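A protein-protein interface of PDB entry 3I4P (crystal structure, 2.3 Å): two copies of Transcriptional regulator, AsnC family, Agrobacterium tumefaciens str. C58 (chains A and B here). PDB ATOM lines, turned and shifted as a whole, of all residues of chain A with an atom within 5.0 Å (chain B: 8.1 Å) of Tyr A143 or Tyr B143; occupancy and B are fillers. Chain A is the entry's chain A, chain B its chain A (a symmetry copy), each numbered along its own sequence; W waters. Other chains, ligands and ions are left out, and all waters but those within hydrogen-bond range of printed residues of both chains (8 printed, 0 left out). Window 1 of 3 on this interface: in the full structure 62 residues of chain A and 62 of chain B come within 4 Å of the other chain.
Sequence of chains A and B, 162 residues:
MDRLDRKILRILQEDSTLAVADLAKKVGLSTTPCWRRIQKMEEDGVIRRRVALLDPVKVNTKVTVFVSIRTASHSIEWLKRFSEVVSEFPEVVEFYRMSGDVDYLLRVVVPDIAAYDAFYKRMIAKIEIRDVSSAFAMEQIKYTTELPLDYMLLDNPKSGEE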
ATOM      1  N   ARG A  48      -4.305   7.263  18.700  1.00  0.00           N
ATOM      2  CA  ARG A  48      -3.550   7.417  19.959  1.00  0.00           C
ATOM      3  C   ARG A  48      -4.083   8.575  20.801  1.00  0.00           C
ATOM      4  O   ARG A  48      -4.104   8.480  22.026  1.00  0.00           O
ATOM      5  CB  ARG A  48      -2.036   7.492  19.763  1.00  0.00           C
ATOM      6  CG  ARG A  48      -1.566   8.181  18.563  1.00  0.00           C
ATOM      7  CD  ARG A  48      -0.069   8.043  18.381  1.00  0.00           C
ATOM      8  NE  ARG A  48       0.464   9.118  17.536  1.00  0.00           N
ATOM      9  CZ  ARG A  48       0.876  10.308  17.980  1.00  0.00           C
ATOM     10  NH1 ARG A  48       0.821  10.610  19.271  1.00  0.00           N
ATOM     11  NH2 ARG A  48       1.361  11.212  17.130  1.00  0.00           N
ATOM     12  N   VAL A  93      10.235  19.842  18.365  1.00  0.00           N
ATOM     13  CA  VAL A  93       8.930  19.281  18.101  1.00  0.00           C
ATOM     14  C   VAL A  93       9.052  17.894  17.465  1.00  0.00           C
ATOM     15  O   VAL A  93       8.098  17.078  17.505  1.00  0.00           O
ATOM     16  CB  VAL A  93       8.012  20.262  17.343  1.00  0.00           C
ATOM     17  CG1 VAL A  93       7.596  21.435  18.281  1.00  0.00           C
ATOM     18  CG2 VAL A  93       8.635  20.716  16.072  1.00  0.00           C
ATOM     19  N   GLU A  94      10.231  17.609  16.906  1.00  0.00           N
ATOM     20  CA  GLU A  94      10.496  16.307  16.307  1.00  0.00           C
ATOM     21  C   GLU A  94      11.938  16.012  16.537  1.00  0.00           C
ATOM     22  O   GLU A  94      12.759  16.905  16.495  1.00  0.00           O
ATOM     23  CB  GLU A  94      10.176  16.278  14.799  1.00  0.00           C
ATOM     24  CG  GLU A  94       8.751  16.511  14.484  1.00  0.00           C
ATOM     25  CD  GLU A  94       8.434  16.576  12.961  1.00  0.00           C
ATOM     26  OE1 GLU A  94       9.083  15.867  12.177  1.00  0.00           O
ATOM     27  OE2 GLU A  94       7.504  17.340  12.607  1.00  0.00           O
ATOM     28  N   TYR A  96      14.809  12.705  15.895  1.00  0.00           N
ATOM     29  CA  TYR A  96      15.088  11.410  15.294  1.00  0.00           C
ATOM     30  C   TYR A  96      16.516  11.024  15.459  1.00  0.00           C
ATOM     31  O   TYR A  96      17.435  11.847  15.289  1.00  0.00           O
ATOM     32  CB  TYR A  96      14.809  11.400  13.768  1.00  0.00           C
ATOM     33  CG  TYR A  96      13.385  11.668  13.429  1.00  0.00           C
ATOM     34  CD1 TYR A  96      12.471  10.638  13.279  1.00  0.00           C
ATOM     35  CD2 TYR A  96      12.934  12.966  13.312  1.00  0.00           C
ATOM     36  CE1 TYR A  96      11.167  10.910  12.994  1.00  0.00           C
ATOM     37  CE2 TYR A  96      11.631  13.243  13.062  1.00  0.00           C
ATOM     38  CZ  TYR A  96      10.752  12.225  12.901  1.00  0.00           C
ATOM     39  OH  TYR A  96       9.443  12.549  12.639  1.00  0.00           O
ATOM     40  N   ARG A 107      13.787  18.877  14.565  1.00  0.00           N
ATOM     41  CA  ARG A 107      13.024  20.025  14.067  1.00  0.00           C
ATOM     42  C   ARG A 107      12.626  20.913  15.227  1.00  0.00           C
ATOM     43  O   ARG A 107      12.001  20.446  16.194  1.00  0.00           O
ATOM     44  CB  ARG A 107      11.754  19.610  13.347  1.00  0.00           C
ATOM     45  CG  ARG A 107      11.111  20.772  12.654  1.00  0.00           C
ATOM     46  CD  ARG A 107      10.049  20.377  11.621  1.00  0.00           C
ATOM     47  NE  ARG A 107       8.758  20.104  12.238  1.00  0.00           N
ATOM     48  CZ  ARG A 107       7.810  20.994  12.564  1.00  0.00           C
ATOM     49  NH1 ARG A 107       6.689  20.556  13.120  1.00  0.00           N
ATOM     50  NH2 ARG A 107       7.945  22.287  12.372  1.00  0.00           N
ATOM     51  N   GLN A 140       7.400  26.662   5.050  1.00  0.00           N
ATOM     52  CA  GLN A 140       6.695  25.399   5.236  1.00  0.00           C
ATOM     53  C   GLN A 140       5.624  25.237   4.151  1.00  0.00           C
ATOM     54  O   GLN A 140       4.542  25.828   4.238  1.00  0.00           O
ATOM     55  CB  GLN A 140       6.074  25.358   6.614  1.00  0.00           C
ATOM     56  CG  GLN A 140       5.506  24.033   7.054  1.00  0.00           C
ATOM     57  CD  GLN A 140       4.897  24.170   8.466  1.00  0.00           C
ATOM     58  OE1 GLN A 140       3.852  24.819   8.636  1.00  0.00           O
ATOM     59  NE2 GLN A 140       5.561  23.565   9.478  1.00  0.00           N
ATOM     60  N   ILE A 141       5.943  24.454   3.112  1.00  0.00           N
ATOM     61  CA  ILE A 141       5.030  24.242   1.976  1.00  0.00           C
ATOM     62  C   ILE A 141       3.905  23.298   2.353  1.00  0.00           C
ATOM     63  O   ILE A 141       2.760  23.577   2.067  1.00  0.00           O
ATOM     64  CB  ILE A 141       5.741  23.677   0.728  1.00  0.00           C
ATOM     65  CG1 ILE A 141       6.804  24.665   0.231  1.00  0.00           C
ATOM     66  CG2 ILE A 141       4.683  23.395  -0.382  1.00  0.00           C
ATOM     67  CD1 ILE A 141       7.895  24.041  -0.581  1.00  0.00           C
ATOM     68  N   LYS A 142       4.234  22.199   3.033  1.00  0.00           N
ATOM     69  CA  LYS A 142       3.215  21.270   3.555  1.00  0.00           C
ATOM     70  C   LYS A 142       3.586  20.851   4.965  1.00  0.00           C
ATOM     71  O   LYS A 142       4.721  20.523   5.231  1.00  0.00           O
ATOM     72  CB  LYS A 142       3.090  20.015   2.655  1.00  0.00           C
ATOM     73  CG  LYS A 142       2.020  19.022   3.070  1.00  0.00           C
ATOM     74  CD  LYS A 142       2.125  17.772   2.215  1.00  0.00           C
ATOM     75  CE  LYS A 142       0.936  16.836   2.325  1.00  0.00           C
ATOM     76  NZ  LYS A 142       1.157  15.607   1.492  1.00  0.00           N
ATOM     77  N   TYR A 143       2.604  20.826   5.848  1.00  0.00           N
ATOM     78  CA  TYR A 143       2.733  20.145   7.126  1.00  0.00           C
ATOM     79  C   TYR A 143       1.400  19.516   7.489  1.00  0.00           C
ATOM     80  O   TYR A 143       0.426  20.190   7.788  1.00  0.00           O
ATOM     81  CB  TYR A 143       3.267  21.066   8.246  1.00  0.00           C
ATOM     82  CG  TYR A 143       3.175  20.450   9.633  1.00  0.00           C
ATOM     83  CD1 TYR A 143       4.222  19.723  10.174  1.00  0.00           C
ATOM     84  CD2 TYR A 143       2.038  20.599  10.399  1.00  0.00           C
ATOM     85  CE1 TYR A 143       4.128  19.152  11.455  1.00  0.00           C
ATOM     86  CE2 TYR A 143       1.932  20.049  11.659  1.00  0.00           C
ATOM     87  CZ  TYR A 143       2.976  19.319  12.186  1.00  0.00           C
ATOM     88  OH  TYR A 143       2.844  18.782  13.441  1.00  0.00           O
ATOM     89  N   THR A 144       1.397  18.192   7.512  1.00  0.00           N
ATOM     90  CA  THR A 144       0.234  17.445   7.875  1.00  0.00           C
ATOM     91  C   THR A 144       0.586  16.408   8.931  1.00  0.00           C
ATOM     92  O   THR A 144       1.720  15.894   8.975  1.00  0.00           O
ATOM     93  CB  THR A 144      -0.393  16.730   6.627  1.00  0.00           C
ATOM     94  OG1 THR A 144      -1.676  16.226   6.993  1.00  0.00           O
ATOM     95  CG2 THR A 144       0.485  15.590   6.140  1.00  0.00           C
ATOM     96  N   THR A 145      -0.426  16.101   9.746  1.00  0.00           N
ATOM     97  CA  THR A 145      -0.375  15.044  10.768  1.00  0.00           C
ATOM     98  C   THR A 145      -1.102  13.775  10.290  1.00  0.00           C
ATOM     99  O   THR A 145      -1.120  12.755  10.974  1.00  0.00           O
ATOM    100  CB  THR A 145      -1.039  15.598  12.081  1.00  0.00           C
ATOM    101  OG1 THR A 145      -2.436  15.854  11.848  1.00  0.00           O
ATOM    102  CG2 THR A 145      -0.340  16.896  12.509  1.00  0.00           C
ATOM    103  N   ARG B  48      -6.466  25.980  14.332  1.00  0.00           N
ATOM    104  CA  ARG B  48      -6.782  25.836  12.897  1.00  0.00           C
ATOM    105  C   ARG B  48      -7.704  24.645  12.636  1.00  0.00           C
ATOM    106  O   ARG B  48      -8.566  24.721  11.765  1.00  0.00           O
ATOM    107  CB  ARG B  48      -5.549  25.821  11.994  1.00  0.00           C
ATOM    108  CG  ARG B  48      -4.355  25.170  12.529  1.00  0.00           C
ATOM    109  CD  ARG B  48      -3.152  25.368  11.632  1.00  0.00           C
ATOM    110  NE  ARG B  48      -2.142  24.327  11.861  1.00  0.00           N
ATOM    111  CZ  ARG B  48      -2.105  23.147  11.237  1.00  0.00           C
ATOM    112  NH1 ARG B  48      -3.023  22.823  10.334  1.00  0.00           N
ATOM    113  NH2 ARG B  48      -1.133  22.275  11.504  1.00  0.00           N
ATOM    114  N   ARG B  49      -7.522  23.585  13.419  1.00  0.00           N
ATOM    115  CA  ARG B  49      -8.330  22.372  13.344  1.00  0.00           C
ATOM    116  C   ARG B  49      -8.070  21.478  14.545  1.00  0.00           C
ATOM    117  O   ARG B  49      -7.139  21.679  15.309  1.00  0.00           O
ATOM    118  CB  ARG B  49      -8.028  21.583  12.054  1.00  0.00           C
ATOM    119  CG  ARG B  49      -6.647  20.898  11.990  1.00  0.00           C
ATOM    120  CD  ARG B  49      -6.541  20.079  10.763  1.00  0.00           C
ATOM    121  NE  ARG B  49      -6.499  20.950   9.609  1.00  0.00           N
ATOM    122  CZ  ARG B  49      -6.734  20.570   8.359  1.00  0.00           C
ATOM    123  NH1 ARG B  49      -7.059  19.305   8.063  1.00  0.00           N
ATOM    124  NH2 ARG B  49      -6.672  21.482   7.399  1.00  0.00           N
ATOM    125  N   LEU B  53      -4.825  11.724  15.862  1.00  0.00           N
ATOM    126  CA  LEU B  53      -3.442  11.383  15.545  1.00  0.00           C
ATOM    127  C   LEU B  53      -3.363   9.875  15.654  1.00  0.00           C
ATOM    128  O   LEU B  53      -3.806   9.296  16.644  1.00  0.00           O
ATOM    129  CB  LEU B  53      -2.482  12.022  16.551  1.00  0.00           C
ATOM    130  CG  LEU B  53      -2.396  13.538  16.558  1.00  0.00           C
ATOM    131  CD1 LEU B  53      -1.192  14.029  17.466  1.00  0.00           C
ATOM    132  CD2 LEU B  53      -2.270  14.053  15.128  1.00  0.00           C
ATOM    133  N   LEU B  54      -2.802   9.236  14.642  1.00  0.00           N
ATOM    134  CA  LEU B  54      -2.739   7.791  14.646  1.00  0.00           C
ATOM    135  C   LEU B  54      -1.343   7.316  14.943  1.00  0.00           C
ATOM    136  O   LEU B  54      -0.378   8.065  14.799  1.00  0.00           O
ATOM    137  CB  LEU B  54      -3.194   7.255  13.290  1.00  0.00           C
ATOM    138  CG  LEU B  54      -4.509   7.809  12.764  1.00  0.00           C
ATOM    139  CD1 LEU B  54      -4.772   7.147  11.430  1.00  0.00           C
ATOM    140  CD2 LEU B  54      -5.631   7.598  13.770  1.00  0.00           C
ATOM    141  N   PRO B  56       1.766   5.338  13.939  1.00  0.00           N
ATOM    142  CA  PRO B  56       2.380   4.926  12.668  1.00  0.00           C
ATOM    143  C   PRO B  56       2.715   3.427  12.599  1.00  0.00           C
ATOM    144  O   PRO B  56       2.612   2.819  11.526  1.00  0.00           O
ATOM    145  CB  PRO B  56       3.651   5.771  12.603  1.00  0.00           C
ATOM    146  CG  PRO B  56       3.895   6.252  14.018  1.00  0.00           C
ATOM    147  CD  PRO B  56       2.558   6.372  14.647  1.00  0.00           C
ATOM    148  N   THR B  64      10.454   6.490   8.720  1.00  0.00           N
ATOM    149  CA  THR B  64      10.601   7.875   8.302  1.00  0.00           C
ATOM    150  C   THR B  64      11.885   8.024   7.467  1.00  0.00           C
ATOM    151  O   THR B  64      12.951   7.566   7.842  1.00  0.00           O
ATOM    152  CB  THR B  64      10.704   8.842   9.528  1.00  0.00           C
ATOM    153  OG1 THR B  64       9.482   8.809  10.266  1.00  0.00           O
ATOM    154  CG2 THR B  64      10.965  10.251   9.084  1.00  0.00           C
ATOM    155  N   SER B  87       3.516  17.963  -2.981  1.00  0.00           N
ATOM    156  CA  SER B  87       2.504  18.091  -1.917  1.00  0.00           C
ATOM    157  C   SER B  87       1.352  17.106  -2.027  1.00  0.00           C
ATOM    158  O   SER B  87       0.753  16.759  -1.011  1.00  0.00           O
ATOM    159  CB  SER B  87       1.931  19.510  -1.852  1.00  0.00           C
ATOM    160  OG  SER B  87       2.884  20.374  -1.287  1.00  0.00           O
ATOM    161  N   VAL B  92       4.239  12.252   1.692  1.00  0.00           N
ATOM    162  CA  VAL B  92       5.070  13.415   2.026  1.00  0.00           C
ATOM    163  C   VAL B  92       4.312  14.158   3.123  1.00  0.00           C
ATOM    164  O   VAL B  92       3.295  14.845   2.862  1.00  0.00           O
ATOM    165  CB  VAL B  92       5.321  14.335   0.815  1.00  0.00           C
ATOM    166  CG1 VAL B  92       6.104  15.602   1.240  1.00  0.00           C
ATOM    167  CG2 VAL B  92       5.977  13.531  -0.313  1.00  0.00           C
ATOM    168  N   VAL B  93       4.766  13.972   4.362  1.00  0.00           N
ATOM    169  CA  VAL B  93       3.983  14.487   5.461  1.00  0.00           C
ATOM    170  C   VAL B  93       4.457  15.888   5.859  1.00  0.00           C
ATOM    171  O   VAL B  93       3.707  16.666   6.501  1.00  0.00           O
ATOM    172  CB  VAL B  93       3.878  13.483   6.628  1.00  0.00           C
ATOM    173  CG1 VAL B  93       2.976  12.282   6.217  1.00  0.00           C
ATOM    174  CG2 VAL B  93       5.223  13.073   7.113  1.00  0.00           C
ATOM    175  N   GLU B  94       5.684  16.226   5.456  1.00  0.00           N
ATOM    176  CA  GLU B  94       6.238  17.546   5.728  1.00  0.00           C
ATOM    177  C   GLU B  94       7.112  17.893   4.572  1.00  0.00           C
ATOM    178  O   GLU B  94       7.769  17.033   4.023  1.00  0.00           O
ATOM    179  CB  GLU B  94       7.045  17.586   7.041  1.00  0.00           C
ATOM    180  CG  GLU B  94       6.240  17.304   8.247  1.00  0.00           C
ATOM    181  CD  GLU B  94       7.063  17.250   9.568  1.00  0.00           C
ATOM    182  OE1 GLU B  94       8.045  17.995   9.700  1.00  0.00           O
ATOM    183  OE2 GLU B  94       6.662  16.456  10.454  1.00  0.00           O
ATOM    184  N   PHE B  95       7.139  19.169   4.231  1.00  0.00           N
ATOM    185  CA  PHE B  95       7.790  19.632   2.998  1.00  0.00           C
ATOM    186  C   PHE B  95       8.198  21.073   3.200  1.00  0.00           C
ATOM    187  O   PHE B  95       7.335  21.947   3.450  1.00  0.00           O
ATOM    188  CB  PHE B  95       6.780  19.484   1.856  1.00  0.00           C
ATOM    189  CG  PHE B  95       7.269  19.900   0.493  1.00  0.00           C
ATOM    190  CD1 PHE B  95       8.612  19.943   0.154  1.00  0.00           C
ATOM    191  CD2 PHE B  95       6.343  20.163  -0.492  1.00  0.00           C
ATOM    192  CE1 PHE B  95       9.018  20.280  -1.152  1.00  0.00           C
ATOM    193  CE2 PHE B  95       6.747  20.528  -1.785  1.00  0.00           C
ATOM    194  CZ  PHE B  95       8.086  20.565  -2.114  1.00  0.00           C
ATOM    195  N   TYR B  96       9.506  21.316   3.109  1.00  0.00           N
ATOM    196  CA  TYR B  96      10.072  22.630   3.372  1.00  0.00           C
ATOM    197  C   TYR B  96      10.977  23.067   2.273  1.00  0.00           C
ATOM    198  O   TYR B  96      11.791  22.283   1.751  1.00  0.00           O
ATOM    199  CB  TYR B  96      10.922  22.653   4.669  1.00  0.00           C
ATOM    200  CG  TYR B  96      10.135  22.335   5.892  1.00  0.00           C
ATOM    201  CD1 TYR B  96       9.538  23.332   6.646  1.00  0.00           C
ATOM    202  CD2 TYR B  96       9.939  21.023   6.269  1.00  0.00           C
ATOM    203  CE1 TYR B  96       8.801  23.015   7.747  1.00  0.00           C
ATOM    204  CE2 TYR B  96       9.179  20.701   7.343  1.00  0.00           C
ATOM    205  CZ  TYR B  96       8.615  21.686   8.081  1.00  0.00           C
ATOM    206  OH  TYR B  96       7.861  21.317   9.167  1.00  0.00           O
ATOM    207  N   ARG B 107       9.919  15.131   4.682  1.00  0.00           N
ATOM    208  CA  ARG B 107       9.753  13.962   5.551  1.00  0.00           C
ATOM    209  C   ARG B 107       8.700  13.042   4.971  1.00  0.00           C
ATOM    210  O   ARG B 107       7.563  13.470   4.709  1.00  0.00           O
ATOM    211  CB  ARG B 107       9.315  14.339   6.954  1.00  0.00           C
ATOM    212  CG  ARG B 107       9.372  13.164   7.881  1.00  0.00           C
ATOM    213  CD  ARG B 107       9.300  13.534   9.368  1.00  0.00           C
ATOM    214  NE  ARG B 107       7.930  13.748   9.815  1.00  0.00           N
ATOM    215  CZ  ARG B 107       7.053  12.818  10.219  1.00  0.00           C
ATOM    216  NH1 ARG B 107       5.842  13.203  10.595  1.00  0.00           N
ATOM    217  NH2 ARG B 107       7.333  11.534  10.244  1.00  0.00           N
ATOM    218  N   VAL B 109       6.896   9.076   5.099  1.00  0.00           N
ATOM    219  CA  VAL B 109       6.612   7.877   5.918  1.00  0.00           C
ATOM    220  C   VAL B 109       6.087   6.711   5.018  1.00  0.00           C
ATOM    221  O   VAL B 109       5.268   6.901   4.098  1.00  0.00           O
ATOM    222  CB  VAL B 109       5.661   8.203   7.123  1.00  0.00           C
ATOM    223  CG1 VAL B 109       6.320   9.277   8.081  1.00  0.00           C
ATOM    224  CG2 VAL B 109       4.333   8.691   6.632  1.00  0.00           C
ATOM    225  N   GLN B 140      12.151   7.254  15.858  1.00  0.00           N
ATOM    226  CA  GLN B 140      11.465   8.486  16.228  1.00  0.00           C
ATOM    227  C   GLN B 140      11.432   8.623  17.755  1.00  0.00           C
ATOM    228  O   GLN B 140      10.612   7.990  18.429  1.00  0.00           O
ATOM    229  CB  GLN B 140      10.065   8.482  15.659  1.00  0.00           C
ATOM    230  CG  GLN B 140       9.299   9.777  15.752  1.00  0.00           C
ATOM    231  CD  GLN B 140       7.892   9.596  15.146  1.00  0.00           C
ATOM    232  OE1 GLN B 140       7.043   8.904  15.733  1.00  0.00           O
ATOM    233  NE2 GLN B 140       7.651  10.210  13.965  1.00  0.00           N
ATOM    234  N   ILE B 141      12.349   9.433  18.299  1.00  0.00           N
ATOM    235  CA  ILE B 141      12.462   9.628  19.755  1.00  0.00           C
ATOM    236  C   ILE B 141      11.353  10.522  20.271  1.00  0.00           C
ATOM    237  O   ILE B 141      10.732  10.204  21.264  1.00  0.00           O
ATOM    238  CB  ILE B 141      13.815  10.239  20.178  1.00  0.00           C
ATOM    239  CG1 ILE B 141      14.965   9.300  19.790  1.00  0.00           C
ATOM    240  CG2 ILE B 141      13.804  10.497  21.716  1.00  0.00           C
ATOM    241  CD1 ILE B 141      16.290   9.978  19.637  1.00  0.00           C
ATOM    242  N   LYS B 142      11.080  11.623  19.569  1.00  0.00           N
ATOM    243  CA  LYS B 142       9.948  12.504  19.907  1.00  0.00           C
ATOM    244  C   LYS B 142       9.229  12.915  18.637  1.00  0.00           C
ATOM    245  O   LYS B 142       9.854  13.282  17.666  1.00  0.00           O
ATOM    246  CB  LYS B 142      10.430  13.767  20.664  1.00  0.00           C
ATOM    247  CG  LYS B 142       9.331  14.712  21.116  1.00  0.00           C
ATOM    248  CD  LYS B 142       9.949  15.977  21.683  1.00  0.00           C
ATOM    249  CE  LYS B 142       8.977  16.866  22.437  1.00  0.00           C
ATOM    250  NZ  LYS B 142       9.664  18.115  22.907  1.00  0.00           N
ATOM    251  N   TYR B 143       7.908  12.889  18.674  1.00  0.00           N
ATOM    252  CA  TYR B 143       7.095  13.555  17.670  1.00  0.00           C
ATOM    253  C   TYR B 143       5.856  14.127  18.335  1.00  0.00           C
ATOM    254  O   TYR B 143       4.971  13.412  18.779  1.00  0.00           O
ATOM    255  CB  TYR B 143       6.744  12.638  16.476  1.00  0.00           C
ATOM    256  CG  TYR B 143       5.698  13.229  15.544  1.00  0.00           C
ATOM    257  CD1 TYR B 143       6.056  13.987  14.442  1.00  0.00           C
ATOM    258  CD2 TYR B 143       4.354  13.025  15.771  1.00  0.00           C
ATOM    259  CE1 TYR B 143       5.083  14.534  13.588  1.00  0.00           C
ATOM    260  CE2 TYR B 143       3.388  13.551  14.940  1.00  0.00           C
ATOM    261  CZ  TYR B 143       3.752  14.313  13.849  1.00  0.00           C
ATOM    262  OH  TYR B 143       2.771  14.824  13.039  1.00  0.00           O
ATOM    263  N   THR B 144       5.788  15.449  18.341  1.00  0.00           N
ATOM    264  CA  THR B 144       4.667  16.146  18.890  1.00  0.00           C
ATOM    265  C   THR B 144       4.154  17.179  17.899  1.00  0.00           C
ATOM    266  O   THR B 144       4.925  17.736  17.094  1.00  0.00           O
ATOM    267  CB  THR B 144       5.046  16.855  20.238  1.00  0.00           C
ATOM    268  OG1 THR B 144       3.846  17.305  20.865  1.00  0.00           O
ATOM    269  CG2 THR B 144       5.974  18.036  20.003  1.00  0.00           C
ATOM    270  N   THR B 145       2.849  17.435  18.010  1.00  0.00           N
ATOM    271  CA  THR B 145       2.141  18.477  17.251  1.00  0.00           C
ATOM    272  C   THR B 145       1.896  19.725  18.118  1.00  0.00           C
ATOM    273  O   THR B 145       1.373  20.733  17.651  1.00  0.00           O
ATOM    274  CB  THR B 145       0.777  17.879  16.749  1.00  0.00           C
ATOM    275  OG1 THR B 145      -0.064  17.572  17.876  1.00  0.00           O
ATOM    276  CG2 THR B 145       1.038  16.601  15.937  1.00  0.00           C
ATOM    277  N   GLU B 146       2.278  19.625  19.394  1.00  0.00           N
ATOM    278  CA  GLU B 146       2.306  20.760  20.349  1.00  0.00           C
ATOM    279  C   GLU B 146       3.413  21.748  20.004  1.00  0.00           C
ATOM    280  O   GLU B 146       4.601  21.404  19.961  1.00  0.00           O
ATOM    281  CB  GLU B 146       2.519  20.266  21.782  1.00  0.00           C
ATOM    282  CG  GLU B 146       1.380  19.380  22.269  1.00  0.00           C
ATOM    283  CD  GLU B 146       1.704  18.572  23.511  1.00  0.00           C
ATOM    284  OE1 GLU B 146       2.586  19.002  24.291  1.00  0.00           O
ATOM    285  OE2 GLU B 146       1.074  17.517  23.736  1.00  0.00           O
ATOM    286  N   LEU B 147       3.011  22.978  19.755  1.00  0.00           N
ATOM    287  CA  LEU B 147       3.933  24.084  19.620  1.00  0.00           C
ATOM    288  C   LEU B 147       4.358  24.610  21.009  1.00  0.00           C
ATOM    289  O   LEU B 147       3.614  24.516  21.972  1.00  0.00           O
ATOM    290  CB  LEU B 147       3.297  25.202  18.772  1.00  0.00           C
ATOM    291  CG  LEU B 147       2.893  24.786  17.329  1.00  0.00           C
ATOM    292  CD1 LEU B 147       2.178  25.927  16.614  1.00  0.00           C
ATOM    293  CD2 LEU B 147       4.124  24.265  16.506  1.00  0.00           C
HETATM  294  O   HOH W   1       0.713  10.429  14.297  1.00  0.00           O
HETATM  295  O   HOH W   2      -2.323  10.828  12.140  1.00  0.00           O
HETATM  296  O   HOH W   3      -1.664  20.069   9.882  1.00  0.00           O
HETATM  297  O   HOH W   4       2.011  13.420  18.705  1.00  0.00           O
HETATM  298  O   HOH W   5       0.907  12.338  12.592  1.00  0.00           O
HETATM  299  O   HOH W   6       1.709  21.202  15.088  1.00  0.00           O
HETATM  300  O   HOH W   7       3.905  15.317  10.534  1.00  0.00           O
HETATM  301  O   HOH W   8       5.410  18.372  14.467  1.00  0.00           O
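The backbone NH (N) of Arg A48 lies within hydrogen-bond range of the backbone carbonyl oxygen (O) of Leu B53 (2.9 Å). The guanidinium group (NE) of Arg A48 is in hydrogen-bond range of the backbone carbonyl oxygen (O) of Leu B54 (3.1 Å). The backbone carbonyl oxygen of Val A93 sits at hydrogen-bond distance from the backbone NH of Thr B144, at 2.9 Å. The side-chain carboxylate of Glu B94 lies close to the side-chain carboxylate of Glu A94 (2.5 Å). OE1 of Glu A94 is in salt-bridge range of NE of Arg B107 (3.4 Å). OH of Tyr A96 is in hydrogen-bond range of NH2 of Arg B107, at 3.3 Å. OH of Tyr A96 lies within hydrogen-bond range of NE2 of Gln B140 (3.2 Å). The guanidinium group (NE) of Arg A107 lies within salt-bridge range of the side-chain carboxylate (OE1) of Glu B94 (3.4 Å). The guanidinium group (NH2) of Arg A107 lies within hydrogen-bond range of the side-chain hydroxyl (OH) of Tyr B96. The side-chain hydroxyl (OH) of Tyr B96 sits at hydrogen-bond distance from the side-chain amide nitrogen (NE2) of Gln A140. The backbone carbonyl oxygen of Phe B95 is in hydrogen-bond range of the backbone NH of Ile A141 (2.9 Å). O of Ser B87 sits at hydrogen-bond distance from NZ of Lys A142 (2.8 Å). NZ of Lys A142 lies within hydrogen-bond range of O of Val B92, 2.7 Å away. O of Lys A142 sits at hydrogen-bond distance from N of Phe B95, at 2.9 Å. O of Val B93 is in hydrogen-bond range of N of Thr A144 (2.9 Å).
The side-chain hydroxyl (OG1) of Thr B144 lies within hydrogen-bond range of the backbone NH (N) of Glu B146 (3.2 Å).
Glu A94 touches Tyr B143 (CG to CD1, 3.7 Å). Tyr A96 touches Thr B64. CG2 of Ile A141 touches OG of Ser B87 (3.6 Å). Arg B48 touches Tyr A143. Tyr A143 touches Thr B145 (OH to CG2, 3.8 Å). Tyr B143 touches Thr A145. Thr A145 touches Thr B145.
Printed residues of chain B within 4 Å of Ile A141: Ser B87 and Phe B95. Tyr A143 touches just these residues of chain B: Arg B48 (3.8 Å), Val B93 (3.7 Å), Glu B94 (3.7 Å), Tyr B143 (3.98 Å) and Thr B145 (3.8 Å). Of the printed residues of chain A, Thr B64 touches Tyr A96. Printed residues of chain A within 4 Å of Tyr B143: Arg A48, Val A93, Glu A94, Tyr A143 and Thr A145. The nearest residue of chain A that does not touch Tyr B143 is Tyr A96 (4.1 Å). The nearest printed residue of chain B that does not touch Arg A107 is Thr B144 (5.2 Å).
Of the 22 printed residues of chain B, 17 touch a printed residue of chain A. Hydrophobic or aromatic side chains of chain B within 4 Å of the printed part of chain A: Leu B53, Val B93, Phe B95, Tyr B96 and Tyr B143. Among the printed residues, 32 pairs touch across the chains. Among the printed residues, Asp or Glu carboxylates within 4 Å of a Lys or Arg side-chain nitrogen of the other chain: Glu A94 with Arg B107 (3.4 Å) and Arg A107 with Glu B94 (3.4 Å).
Val A93 touches Tyr B143, and with the chains exchanged Tyr A143 touches Val B93. Tyr A96 touches Arg B107, and with the chains exchanged Arg A107 touches Tyr B96. Tyr B143 touches its own counterpart, Tyr A143.
Water W2 lies within hydrogen-bond range of O of Thr A145 (2.6 Å) and N of Leu B54 (3.0 Å). Water W8 lies within hydrogen-bond range of O of Thr B144 (2.7 Å), OH of Tyr A143 (2.8 Å), NH1 of Arg A107 (2.9 Å) and OE2 of Glu A94 (3.0 Å).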
